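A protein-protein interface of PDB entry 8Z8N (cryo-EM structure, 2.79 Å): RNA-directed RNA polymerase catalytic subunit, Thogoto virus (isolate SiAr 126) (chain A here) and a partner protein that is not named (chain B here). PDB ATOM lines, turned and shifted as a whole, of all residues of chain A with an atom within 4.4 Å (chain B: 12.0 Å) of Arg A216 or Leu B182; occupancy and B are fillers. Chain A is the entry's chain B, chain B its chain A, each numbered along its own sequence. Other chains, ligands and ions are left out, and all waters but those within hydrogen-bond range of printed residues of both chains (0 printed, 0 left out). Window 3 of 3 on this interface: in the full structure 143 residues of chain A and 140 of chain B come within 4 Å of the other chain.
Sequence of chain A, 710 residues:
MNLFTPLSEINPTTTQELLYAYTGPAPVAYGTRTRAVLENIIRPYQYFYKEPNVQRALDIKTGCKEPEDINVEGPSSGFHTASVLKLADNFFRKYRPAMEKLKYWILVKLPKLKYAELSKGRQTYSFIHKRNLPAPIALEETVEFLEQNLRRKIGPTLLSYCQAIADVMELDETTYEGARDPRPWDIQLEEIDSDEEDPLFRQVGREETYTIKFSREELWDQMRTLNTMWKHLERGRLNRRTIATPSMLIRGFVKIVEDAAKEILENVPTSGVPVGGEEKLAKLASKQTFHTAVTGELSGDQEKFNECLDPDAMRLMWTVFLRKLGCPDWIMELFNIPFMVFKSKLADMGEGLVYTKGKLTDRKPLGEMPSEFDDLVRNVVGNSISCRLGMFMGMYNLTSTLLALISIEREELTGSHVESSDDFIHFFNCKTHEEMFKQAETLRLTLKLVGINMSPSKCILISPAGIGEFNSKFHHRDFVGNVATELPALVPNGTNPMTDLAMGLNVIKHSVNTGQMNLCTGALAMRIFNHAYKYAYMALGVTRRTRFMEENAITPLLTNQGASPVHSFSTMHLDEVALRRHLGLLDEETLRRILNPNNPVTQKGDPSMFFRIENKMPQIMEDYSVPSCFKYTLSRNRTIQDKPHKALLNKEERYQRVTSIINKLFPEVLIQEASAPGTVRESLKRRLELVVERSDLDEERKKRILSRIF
OG1 of Thr B181 is in hydrogen-bond range of O of Thr B178, at 2.7 Å.
O of Glu A170 sits at hydrogen-bond distance from NH1 of Arg A216 (3.0 Å).
The guanidinium group (NH1) of Arg A216 lies within salt-bridge range of the side-chain carboxylate (OD1) of Asp A172, 3.1 Å away.
Of chain A, only Met A169, Arg A216, Glu A217 and Trp A220 come within 4 Å of Leu B182.
Met A169 touches just these residues of chain B: Phe B179 (3.7 Å) and Leu B182 (3.9 Å).
Glu A170 touches just these residues of chain B: Gly B176, Thr B178 and Phe B179.
Asp A172 touches none of the printed residues of chain B.
No residue of chain B comes within 4 Å of Ser A215.
Glu A217 touches just these residues of chain B: Leu B182 (3.8 Å) and Arg B185 (2.7 Å).
No residue of chain B comes within 4 Å of Leu A219.
Of the printed residues of chain A, Arg B185 touches Glu A217 (2.7 Å) and Trp A220 (3.99 Å).
Of the printed residues of chain A, Phe B179 touches Met A169 (3.7 Å), Glu A170 (3.5 Å) and Trp A220 (3.6 Å).
Of the printed residues of chain A, Thr B178 touches Glu A170 and Arg A216.
Val B191 touches none of the printed residues of chain A.
The nearest printed residue of chain A that does not touch Leu B182 is Glu A170 (6.5 Å).
The nearest printed residue of chain A that does not touch Gly B176 is Met A169 (7.6 Å).
N of Gly B176 lies close to OE2 of Glu A170 (3.3 Å).
The guanidinium group of Arg B185 lies within salt-bridge range of the side-chain carboxylate of Glu A217, 2.7 Å away.
Printed residues of chain A that touch a printed residue of chain B: Met A169, Glu A170, Arg A216, Glu A217 and Trp A220.
Along chain A the printed residues that touch a printed residue of chain B span positions 169 to 220.
Hydrophobic or aromatic side chains of chain B within 4 Å of the printed part of chain A: Phe B179 and Leu B182.
Among the printed residues, merely in contact across the chains: Met A169 with Phe B179, Met A169 with Leu B182, Glu A170 with Thr B178, Glu A170 with Phe B179, Arg A216 with Thr B178, Arg A216 with Leu B182, Glu A217 with Leu B182, Trp A220 with Phe B179, Trp A220 with Leu B182 and Trp A220 with Arg B185.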
ATOM      1  N   MET A 169      13.671  -6.554 -20.077  1.00  0.00           N
ATOM      2  CA  MET A 169      14.101  -7.834 -19.528  1.00  0.00           C
ATOM      3  C   MET A 169      13.856  -9.012 -20.461  1.00  0.00           C
ATOM      4  O   MET A 169      14.516 -10.045 -20.307  1.00  0.00           O
ATOM      5  CB  MET A 169      13.407  -8.094 -18.190  1.00  0.00           C
ATOM      6  CG  MET A 169      13.801  -7.120 -17.094  1.00  0.00           C
ATOM      7  SD  MET A 169      15.565  -7.189 -16.729  1.00  0.00           S
ATOM      8  CE  MET A 169      15.690  -8.804 -15.971  1.00  0.00           C
ATOM      9  N   GLU A 170      12.931  -8.896 -21.415  1.00  0.00           N
ATOM     10  CA  GLU A 170      12.679 -10.000 -22.333  1.00  0.00           C
ATOM     11  C   GLU A 170      13.677 -10.065 -23.479  1.00  0.00           C
ATOM     12  O   GLU A 170      13.692 -11.064 -24.207  1.00  0.00           O
ATOM     13  CB  GLU A 170      11.261  -9.918 -22.903  1.00  0.00           C
ATOM     14  CG  GLU A 170      10.164 -10.188 -21.890  1.00  0.00           C
ATOM     15  CD  GLU A 170       9.805  -8.959 -21.096  1.00  0.00           C
ATOM     16  OE1 GLU A 170      10.361  -7.887 -21.400  1.00  0.00           O
ATOM     17  OE2 GLU A 170       8.975  -9.061 -20.168  1.00  0.00           O
ATOM     18  N   LEU A 171      14.502  -9.039 -23.662  1.00  0.00           N
ATOM     19  CA  LEU A 171      15.505  -9.073 -24.717  1.00  0.00           C
ATOM     20  C   LEU A 171      16.618 -10.044 -24.348  1.00  0.00           C
ATOM     21  O   LEU A 171      17.138 -10.014 -23.228  1.00  0.00           O
ATOM     22  CB  LEU A 171      16.072  -7.676 -24.958  1.00  0.00           C
ATOM     23  CG  LEU A 171      15.078  -6.514 -24.935  1.00  0.00           C
ATOM     24  CD1 LEU A 171      15.795  -5.197 -25.179  1.00  0.00           C
ATOM     25  CD2 LEU A 171      13.982  -6.724 -25.967  1.00  0.00           C
ATOM     26  N   ASP A 172      16.975 -10.916 -25.293  1.00  0.00           N
ATOM     27  CA  ASP A 172      18.035 -11.889 -25.039  1.00  0.00           C
ATOM     28  C   ASP A 172      19.373 -11.201 -24.811  1.00  0.00           C
ATOM     29  O   ASP A 172      20.131 -11.581 -23.911  1.00  0.00           O
ATOM     30  CB  ASP A 172      18.131 -12.874 -26.204  1.00  0.00           C
ATOM     31  CG  ASP A 172      16.920 -13.778 -26.306  1.00  0.00           C
ATOM     32  OD1 ASP A 172      16.292 -14.050 -25.261  1.00  0.00           O
ATOM     33  OD2 ASP A 172      16.596 -14.217 -27.429  1.00  0.00           O
ATOM     34  N   SER A 215      23.820 -10.000 -21.031  1.00  0.00           N
ATOM     35  CA  SER A 215      22.853 -11.052 -21.296  1.00  0.00           C
ATOM     36  C   SER A 215      21.632 -10.847 -20.407  1.00  0.00           C
ATOM     37  O   SER A 215      21.610  -9.980 -19.532  1.00  0.00           O
ATOM     38  CB  SER A 215      23.472 -12.432 -21.061  1.00  0.00           C
ATOM     39  OG  SER A 215      24.586 -12.642 -21.912  1.00  0.00           O
ATOM     40  N   ARG A 216      20.598 -11.655 -20.649  1.00  0.00           N
ATOM     41  CA  ARG A 216      19.420 -11.583 -19.792  1.00  0.00           C
ATOM     42  C   ARG A 216      19.765 -11.966 -18.361  1.00  0.00           C
ATOM     43  O   ARG A 216      19.312 -11.320 -17.410  1.00  0.00           O
ATOM     44  CB  ARG A 216      18.308 -12.481 -20.335  1.00  0.00           C
ATOM     45  CG  ARG A 216      16.943 -12.176 -19.734  1.00  0.00           C
ATOM     46  CD  ARG A 216      15.993 -13.355 -19.854  1.00  0.00           C
ATOM     47  NE  ARG A 216      16.352 -14.250 -20.946  1.00  0.00           N
ATOM     48  CZ  ARG A 216      15.887 -14.146 -22.184  1.00  0.00           C
ATOM     49  NH1 ARG A 216      15.046 -13.185 -22.528  1.00  0.00           N
ATOM     50  NH2 ARG A 216      16.277 -15.027 -23.099  1.00  0.00           N
ATOM     51  N   GLU A 217      20.580 -13.010 -18.188  1.00  0.00           N
ATOM     52  CA  GLU A 217      20.998 -13.407 -16.849  1.00  0.00           C
ATOM     53  C   GLU A 217      21.895 -12.355 -16.209  1.00  0.00           C
ATOM     54  O   GLU A 217      21.762 -12.063 -15.016  1.00  0.00           O
ATOM     55  CB  GLU A 217      21.704 -14.761 -16.900  1.00  0.00           C
ATOM     56  CG  GLU A 217      20.787 -15.923 -17.247  1.00  0.00           C
ATOM     57  CD  GLU A 217      19.638 -16.080 -16.267  1.00  0.00           C
ATOM     58  OE1 GLU A 217      19.825 -15.783 -15.068  1.00  0.00           O
ATOM     59  OE2 GLU A 217      18.544 -16.499 -16.698  1.00  0.00           O
ATOM     60  N   GLU A 218      22.817 -11.773 -16.982  1.00  0.00           N
ATOM     61  CA  GLU A 218      23.703 -10.752 -16.430  1.00  0.00           C
ATOM     62  C   GLU A 218      22.933  -9.496 -16.042  1.00  0.00           C
ATOM     63  O   GLU A 218      23.169  -8.920 -14.972  1.00  0.00           O
ATOM     64  CB  GLU A 218      24.805 -10.418 -17.434  1.00  0.00           C
ATOM     65  CG  GLU A 218      25.779 -11.556 -17.681  1.00  0.00           C
ATOM     66  CD  GLU A 218      26.848 -11.199 -18.694  1.00  0.00           C
ATOM     67  OE1 GLU A 218      26.757 -10.109 -19.297  1.00  0.00           O
ATOM     68  OE2 GLU A 218      27.779 -12.008 -18.888  1.00  0.00           O
ATOM     69  N   LEU A 219      22.007  -9.055 -16.897  1.00  0.00           N
ATOM     70  CA  LEU A 219      21.186  -7.898 -16.561  1.00  0.00           C
ATOM     71  C   LEU A 219      20.298  -8.191 -15.359  1.00  0.00           C
ATOM     72  O   LEU A 219      20.094  -7.325 -14.500  1.00  0.00           O
ATOM     73  CB  LEU A 219      20.344  -7.480 -17.766  1.00  0.00           C
ATOM     74  CG  LEU A 219      19.398  -6.297 -17.557  1.00  0.00           C
ATOM     75  CD1 LEU A 219      20.174  -5.061 -17.141  1.00  0.00           C
ATOM     76  CD2 LEU A 219      18.586  -6.026 -18.813  1.00  0.00           C
ATOM     77  N   TRP A 220      19.763  -9.411 -15.281  1.00  0.00           N
ATOM     78  CA  TRP A 220      18.969  -9.807 -14.124  1.00  0.00           C
ATOM     79  C   TRP A 220      19.798  -9.750 -12.848  1.00  0.00           C
ATOM     80  O   TRP A 220      19.342  -9.234 -11.823  1.00  0.00           O
ATOM     81  CB  TRP A 220      18.404 -11.212 -14.343  1.00  0.00           C
ATOM     82  CG  TRP A 220      17.550 -11.748 -13.225  1.00  0.00           C
ATOM     83  CD1 TRP A 220      17.613 -12.999 -12.686  1.00  0.00           C
ATOM     84  CD2 TRP A 220      16.492 -11.068 -12.530  1.00  0.00           C
ATOM     85  NE1 TRP A 220      16.675 -13.138 -11.694  1.00  0.00           N
ATOM     86  CE2 TRP A 220      15.972 -11.968 -11.581  1.00  0.00           C
ATOM     87  CE3 TRP A 220      15.938  -9.787 -12.617  1.00  0.00           C
ATOM     88  CZ2 TRP A 220      14.931 -11.628 -10.722  1.00  0.00           C
ATOM     89  CZ3 TRP A 220      14.904  -9.453 -11.765  1.00  0.00           C
ATOM     90  CH2 TRP A 220      14.412 -10.369 -10.830  1.00  0.00           C
ATOM     91  N   VAL B 175       3.484  -7.148 -17.711  1.00  0.00           N
ATOM     92  CA  VAL B 175       4.654  -7.942 -17.361  1.00  0.00           C
ATOM     93  C   VAL B 175       4.740  -9.113 -18.330  1.00  0.00           C
ATOM     94  O   VAL B 175       3.778  -9.872 -18.489  1.00  0.00           O
ATOM     95  CB  VAL B 175       4.574  -8.432 -15.906  1.00  0.00           C
ATOM     96  CG1 VAL B 175       5.768  -9.313 -15.577  1.00  0.00           C
ATOM     97  CG2 VAL B 175       4.498  -7.253 -14.955  1.00  0.00           C
ATOM     98  N   GLY B 176       5.889  -9.260 -18.980  1.00  0.00           N
ATOM     99  CA  GLY B 176       6.046 -10.278 -19.993  1.00  0.00           C
ATOM    100  C   GLY B 176       6.192 -11.665 -19.394  1.00  0.00           C
ATOM    101  O   GLY B 176       6.298 -11.863 -18.182  1.00  0.00           O
ATOM    102  N   THR B 177       6.199 -12.654 -20.287  1.00  0.00           N
ATOM    103  CA  THR B 177       6.317 -14.046 -19.877  1.00  0.00           C
ATOM    104  C   THR B 177       7.741 -14.433 -19.500  1.00  0.00           C
ATOM    105  O   THR B 177       7.928 -15.290 -18.630  1.00  0.00           O
ATOM    106  CB  THR B 177       5.801 -14.971 -20.987  1.00  0.00           C
ATOM    107  OG1 THR B 177       5.801 -16.327 -20.522  1.00  0.00           O
ATOM    108  CG2 THR B 177       6.657 -14.860 -22.243  1.00  0.00           C
ATOM    109  N   THR B 178       8.749 -13.821 -20.127  1.00  0.00           N
ATOM    110  CA  THR B 178      10.130 -14.134 -19.785  1.00  0.00           C
ATOM    111  C   THR B 178      10.528 -13.514 -18.451  1.00  0.00           C
ATOM    112  O   THR B 178      11.199 -14.159 -17.638  1.00  0.00           O
ATOM    113  CB  THR B 178      11.067 -13.658 -20.894  1.00  0.00           C
ATOM    114  OG1 THR B 178      10.644 -14.211 -22.147  1.00  0.00           O
ATOM    115  CG2 THR B 178      12.491 -14.101 -20.612  1.00  0.00           C
ATOM    116  N   PHE B 179      10.122 -12.265 -18.212  1.00  0.00           N
ATOM    117  CA  PHE B 179      10.394 -11.631 -16.927  1.00  0.00           C
ATOM    118  C   PHE B 179       9.649 -12.323 -15.794  1.00  0.00           C
ATOM    119  O   PHE B 179      10.133 -12.341 -14.656  1.00  0.00           O
ATOM    120  CB  PHE B 179      10.016 -10.151 -16.983  1.00  0.00           C
ATOM    121  CG  PHE B 179      10.556  -9.342 -15.839  1.00  0.00           C
ATOM    122  CD1 PHE B 179      11.755  -9.682 -15.236  1.00  0.00           C
ATOM    123  CD2 PHE B 179       9.861  -8.244 -15.365  1.00  0.00           C
ATOM    124  CE1 PHE B 179      12.250  -8.939 -14.183  1.00  0.00           C
ATOM    125  CE2 PHE B 179      10.352  -7.498 -14.313  1.00  0.00           C
ATOM    126  CZ  PHE B 179      11.547  -7.846 -13.722  1.00  0.00           C
ATOM    127  N   ARG B 180       8.477 -12.890 -16.082  1.00  0.00           N
ATOM    128  CA  ARG B 180       7.701 -13.563 -15.047  1.00  0.00           C
ATOM    129  C   ARG B 180       8.424 -14.799 -14.525  1.00  0.00           C
ATOM    130  O   ARG B 180       8.399 -15.076 -13.320  1.00  0.00           O
ATOM    131  CB  ARG B 180       6.320 -13.925 -15.590  1.00  0.00           C
ATOM    132  CG  ARG B 180       5.281 -14.191 -14.521  1.00  0.00           C
ATOM    133  CD  ARG B 180       3.906 -14.382 -15.132  1.00  0.00           C
ATOM    134  NE  ARG B 180       3.396 -13.137 -15.695  1.00  0.00           N
ATOM    135  CZ  ARG B 180       2.426 -12.412 -15.156  1.00  0.00           C
ATOM    136  NH1 ARG B 180       1.828 -12.781 -14.036  1.00  0.00           N
ATOM    137  NH2 ARG B 180       2.047 -11.287 -15.757  1.00  0.00           N
ATOM    138  N   THR B 181       9.067 -15.560 -15.415  1.00  0.00           N
ATOM    139  CA  THR B 181       9.836 -16.720 -14.974  1.00  0.00           C
ATOM    140  C   THR B 181      11.043 -16.301 -14.144  1.00  0.00           C
ATOM    141  O   THR B 181      11.379 -16.960 -13.152  1.00  0.00           O
ATOM    142  CB  THR B 181      10.279 -17.551 -16.178  1.00  0.00           C
ATOM    143  OG1 THR B 181      11.232 -16.809 -16.950  1.00  0.00           O
ATOM    144  CG2 THR B 181       9.085 -17.901 -17.051  1.00  0.00           C
ATOM    145  N   LEU B 182      11.711 -15.215 -14.538  1.00  0.00           N
ATOM    146  CA  LEU B 182      12.827 -14.701 -13.749  1.00  0.00           C
ATOM    147  C   LEU B 182      12.364 -14.258 -12.368  1.00  0.00           C
ATOM    148  O   LEU B 182      13.069 -14.458 -11.372  1.00  0.00           O
ATOM    149  CB  LEU B 182      13.493 -13.536 -14.480  1.00  0.00           C
ATOM    150  CG  LEU B 182      14.368 -13.850 -15.693  1.00  0.00           C
ATOM    151  CD1 LEU B 182      14.802 -12.565 -16.374  1.00  0.00           C
ATOM    152  CD2 LEU B 182      15.576 -14.664 -15.280  1.00  0.00           C
ATOM    153  N   LEU B 183      11.179 -13.653 -12.293  1.00  0.00           N
ATOM    154  CA  LEU B 183      10.692 -13.108 -11.032  1.00  0.00           C
ATOM    155  C   LEU B 183      10.363 -14.202 -10.025  1.00  0.00           C
ATOM    156  O   LEU B 183      10.435 -13.967  -8.813  1.00  0.00           O
ATOM    157  CB  LEU B 183       9.460 -12.243 -11.290  1.00  0.00           C
ATOM    158  CG  LEU B 183       9.672 -10.739 -11.461  1.00  0.00           C
ATOM    159  CD1 LEU B 183       8.349 -10.047 -11.735  1.00  0.00           C
ATOM    160  CD2 LEU B 183      10.346 -10.147 -10.241  1.00  0.00           C
ATOM    161  N   LYS B 184      10.009 -15.396 -10.495  1.00  0.00           N
ATOM    162  CA  LYS B 184       9.513 -16.463  -9.636  1.00  0.00           C
ATOM    163  C   LYS B 184      10.571 -17.508  -9.303  1.00  0.00           C
ATOM    164  O   LYS B 184      10.229 -18.566  -8.766  1.00  0.00           O
ATOM    165  CB  LYS B 184       8.305 -17.140 -10.285  1.00  0.00           C
ATOM    166  CG  LYS B 184       7.061 -16.272 -10.335  1.00  0.00           C
ATOM    167  CD  LYS B 184       5.850 -17.069 -10.788  1.00  0.00           C
ATOM    168  CE  LYS B 184       6.048 -17.627 -12.186  1.00  0.00           C
ATOM    169  NZ  LYS B 184       4.846 -18.366 -12.659  1.00  0.00           N
ATOM    170  N   ARG B 185      11.842 -17.244  -9.612  1.00  0.00           N
ATOM    171  CA  ARG B 185      12.882 -18.231  -9.337  1.00  0.00           C
ATOM    172  C   ARG B 185      13.088 -18.449  -7.843  1.00  0.00           C
ATOM    173  O   ARG B 185      13.331 -19.582  -7.414  1.00  0.00           O
ATOM    174  CB  ARG B 185      14.199 -17.814  -9.990  1.00  0.00           C
ATOM    175  CG  ARG B 185      14.182 -17.839 -11.504  1.00  0.00           C
ATOM    176  CD  ARG B 185      15.513 -17.380 -12.070  1.00  0.00           C
ATOM    177  NE  ARG B 185      15.741 -17.897 -13.412  1.00  0.00           N
ATOM    178  CZ  ARG B 185      16.815 -17.635 -14.144  1.00  0.00           C
ATOM    179  NH1 ARG B 185      17.787 -16.859 -13.692  1.00  0.00           N
ATOM    180  NH2 ARG B 185      16.917 -18.164 -15.359  1.00  0.00           N
ATOM    181  N   ASP B 186      12.997 -17.393  -7.041  1.00  0.00           N
ATOM    182  CA  ASP B 186      13.336 -17.450  -5.624  1.00  0.00           C
ATOM    183  C   ASP B 186      12.113 -17.231  -4.743  1.00  0.00           C
ATOM    184  O   ASP B 186      12.194 -16.613  -3.680  1.00  0.00           O
ATOM    185  CB  ASP B 186      14.424 -16.434  -5.288  1.00  0.00           C
ATOM    186  CG  ASP B 186      15.797 -16.876  -5.750  1.00  0.00           C
ATOM    187  OD1 ASP B 186      16.431 -17.689  -5.044  1.00  0.00           O
ATOM    188  OD2 ASP B 186      16.245 -16.410  -6.818  1.00  0.00           O
ATOM    189  N   THR B 187      10.959 -17.735  -5.173  1.00  0.00           N
ATOM    190  CA  THR B 187       9.756 -17.663  -4.356  1.00  0.00           C
ATOM    191  C   THR B 187       8.840 -18.824  -4.713  1.00  0.00           C
ATOM    192  O   THR B 187       8.910 -19.384  -5.810  1.00  0.00           O
ATOM    193  CB  THR B 187       9.024 -16.325  -4.531  1.00  0.00           C
ATOM    194  OG1 THR B 187       7.896 -16.277  -3.649  1.00  0.00           O
ATOM    195  CG2 THR B 187       8.549 -16.155  -5.965  1.00  0.00           C
ATOM    196  N   ASP B 188       7.977 -19.183  -3.763  1.00  0.00           N
ATOM    197  CA  ASP B 188       7.043 -20.286  -3.950  1.00  0.00           C
ATOM    198  C   ASP B 188       5.705 -19.847  -4.524  1.00  0.00           C
ATOM    199  O   ASP B 188       4.949 -20.694  -5.012  1.00  0.00           O
ATOM    200  CB  ASP B 188       6.807 -21.009  -2.620  1.00  0.00           C
ATOM    201  CG  ASP B 188       7.936 -21.953  -2.262  1.00  0.00           C
ATOM    202  OD1 ASP B 188       8.668 -22.380  -3.178  1.00  0.00           O
ATOM    203  OD2 ASP B 188       8.091 -22.268  -1.062  1.00  0.00           O
ATOM    204  N   TRP B 189       5.395 -18.558  -4.475  1.00  0.00           N
ATOM    205  CA  TRP B 189       4.135 -18.034  -4.977  1.00  0.00           C
ATOM    206  C   TRP B 189       4.320 -17.440  -6.370  1.00  0.00           C
ATOM    207  O   TRP B 189       5.434 -17.313  -6.881  1.00  0.00           O
ATOM    208  CB  TRP B 189       3.572 -16.985  -4.014  1.00  0.00           C
ATOM    209  CG  TRP B 189       3.281 -17.525  -2.648  1.00  0.00           C
ATOM    210  CD1 TRP B 189       2.963 -18.810  -2.327  1.00  0.00           C
ATOM    211  CD2 TRP B 189       3.287 -16.794  -1.416  1.00  0.00           C
ATOM    212  NE1 TRP B 189       2.765 -18.927  -0.974  1.00  0.00           N
ATOM    213  CE2 TRP B 189       2.959 -17.702  -0.391  1.00  0.00           C
ATOM    214  CE3 TRP B 189       3.536 -15.461  -1.080  1.00  0.00           C
ATOM    215  CZ2 TRP B 189       2.874 -17.321   0.945  1.00  0.00           C
ATOM    216  CZ3 TRP B 189       3.449 -15.083   0.247  1.00  0.00           C
ATOM    217  CH2 TRP B 189       3.122 -16.010   1.242  1.00  0.00           C
ATOM    218  N   ASP B 190       3.198 -17.079  -6.986  1.00  0.00           N
ATOM    219  CA  ASP B 190       3.209 -16.475  -8.311  1.00  0.00           C
ATOM    220  C   ASP B 190       3.506 -14.982  -8.180  1.00  0.00           C
ATOM    221  O   ASP B 190       3.867 -14.488  -7.108  1.00  0.00           O
ATOM    222  CB  ASP B 190       1.885 -16.736  -9.021  1.00  0.00           C
ATOM    223  CG  ASP B 190       1.676 -18.202  -9.343  1.00  0.00           C
ATOM    224  OD1 ASP B 190       2.438 -19.042  -8.817  1.00  0.00           O
ATOM    225  OD2 ASP B 190       0.750 -18.516 -10.120  1.00  0.00           O
ATOM    226  N   VAL B 191       3.366 -14.243  -9.282  1.00  0.00           N
ATOM    227  CA  VAL B 191       3.543 -12.794  -9.221  1.00  0.00           C
ATOM    228  C   VAL B 191       2.497 -12.175  -8.305  1.00  0.00           C
ATOM    229  O   VAL B 191       2.811 -11.328  -7.461  1.00  0.00           O
ATOM    230  CB  VAL B 191       3.500 -12.184 -10.633  1.00  0.00           C
ATOM    231  CG1 VAL B 191       3.321 -10.680 -10.553  1.00  0.00           C
ATOM    232  CG2 VAL B 191       4.771 -12.523 -11.385  1.00  0.00           C
ATOM    233  N   ILE B 192       1.244 -12.597  -8.442  1.00  0.00           N
ATOM    234  CA  ILE B 192       0.186 -12.233  -7.507  1.00  0.00           C
ATOM    235  C   ILE B 192      -0.003 -13.413  -6.556  1.00  0.00           C
ATOM    236  O   ILE B 192      -0.518 -14.459  -6.981  1.00  0.00           O
ATOM    237  CB  ILE B 192      -1.121 -11.889  -8.234  1.00  0.00           C
ATOM    238  CG1 ILE B 192      -0.962 -10.586  -9.017  1.00  0.00           C
ATOM    239  CG2 ILE B 192      -2.264 -11.762  -7.240  1.00  0.00           C
ATOM    240  CD1 ILE B 192      -1.732 -10.557 -10.317  1.00  0.00           C
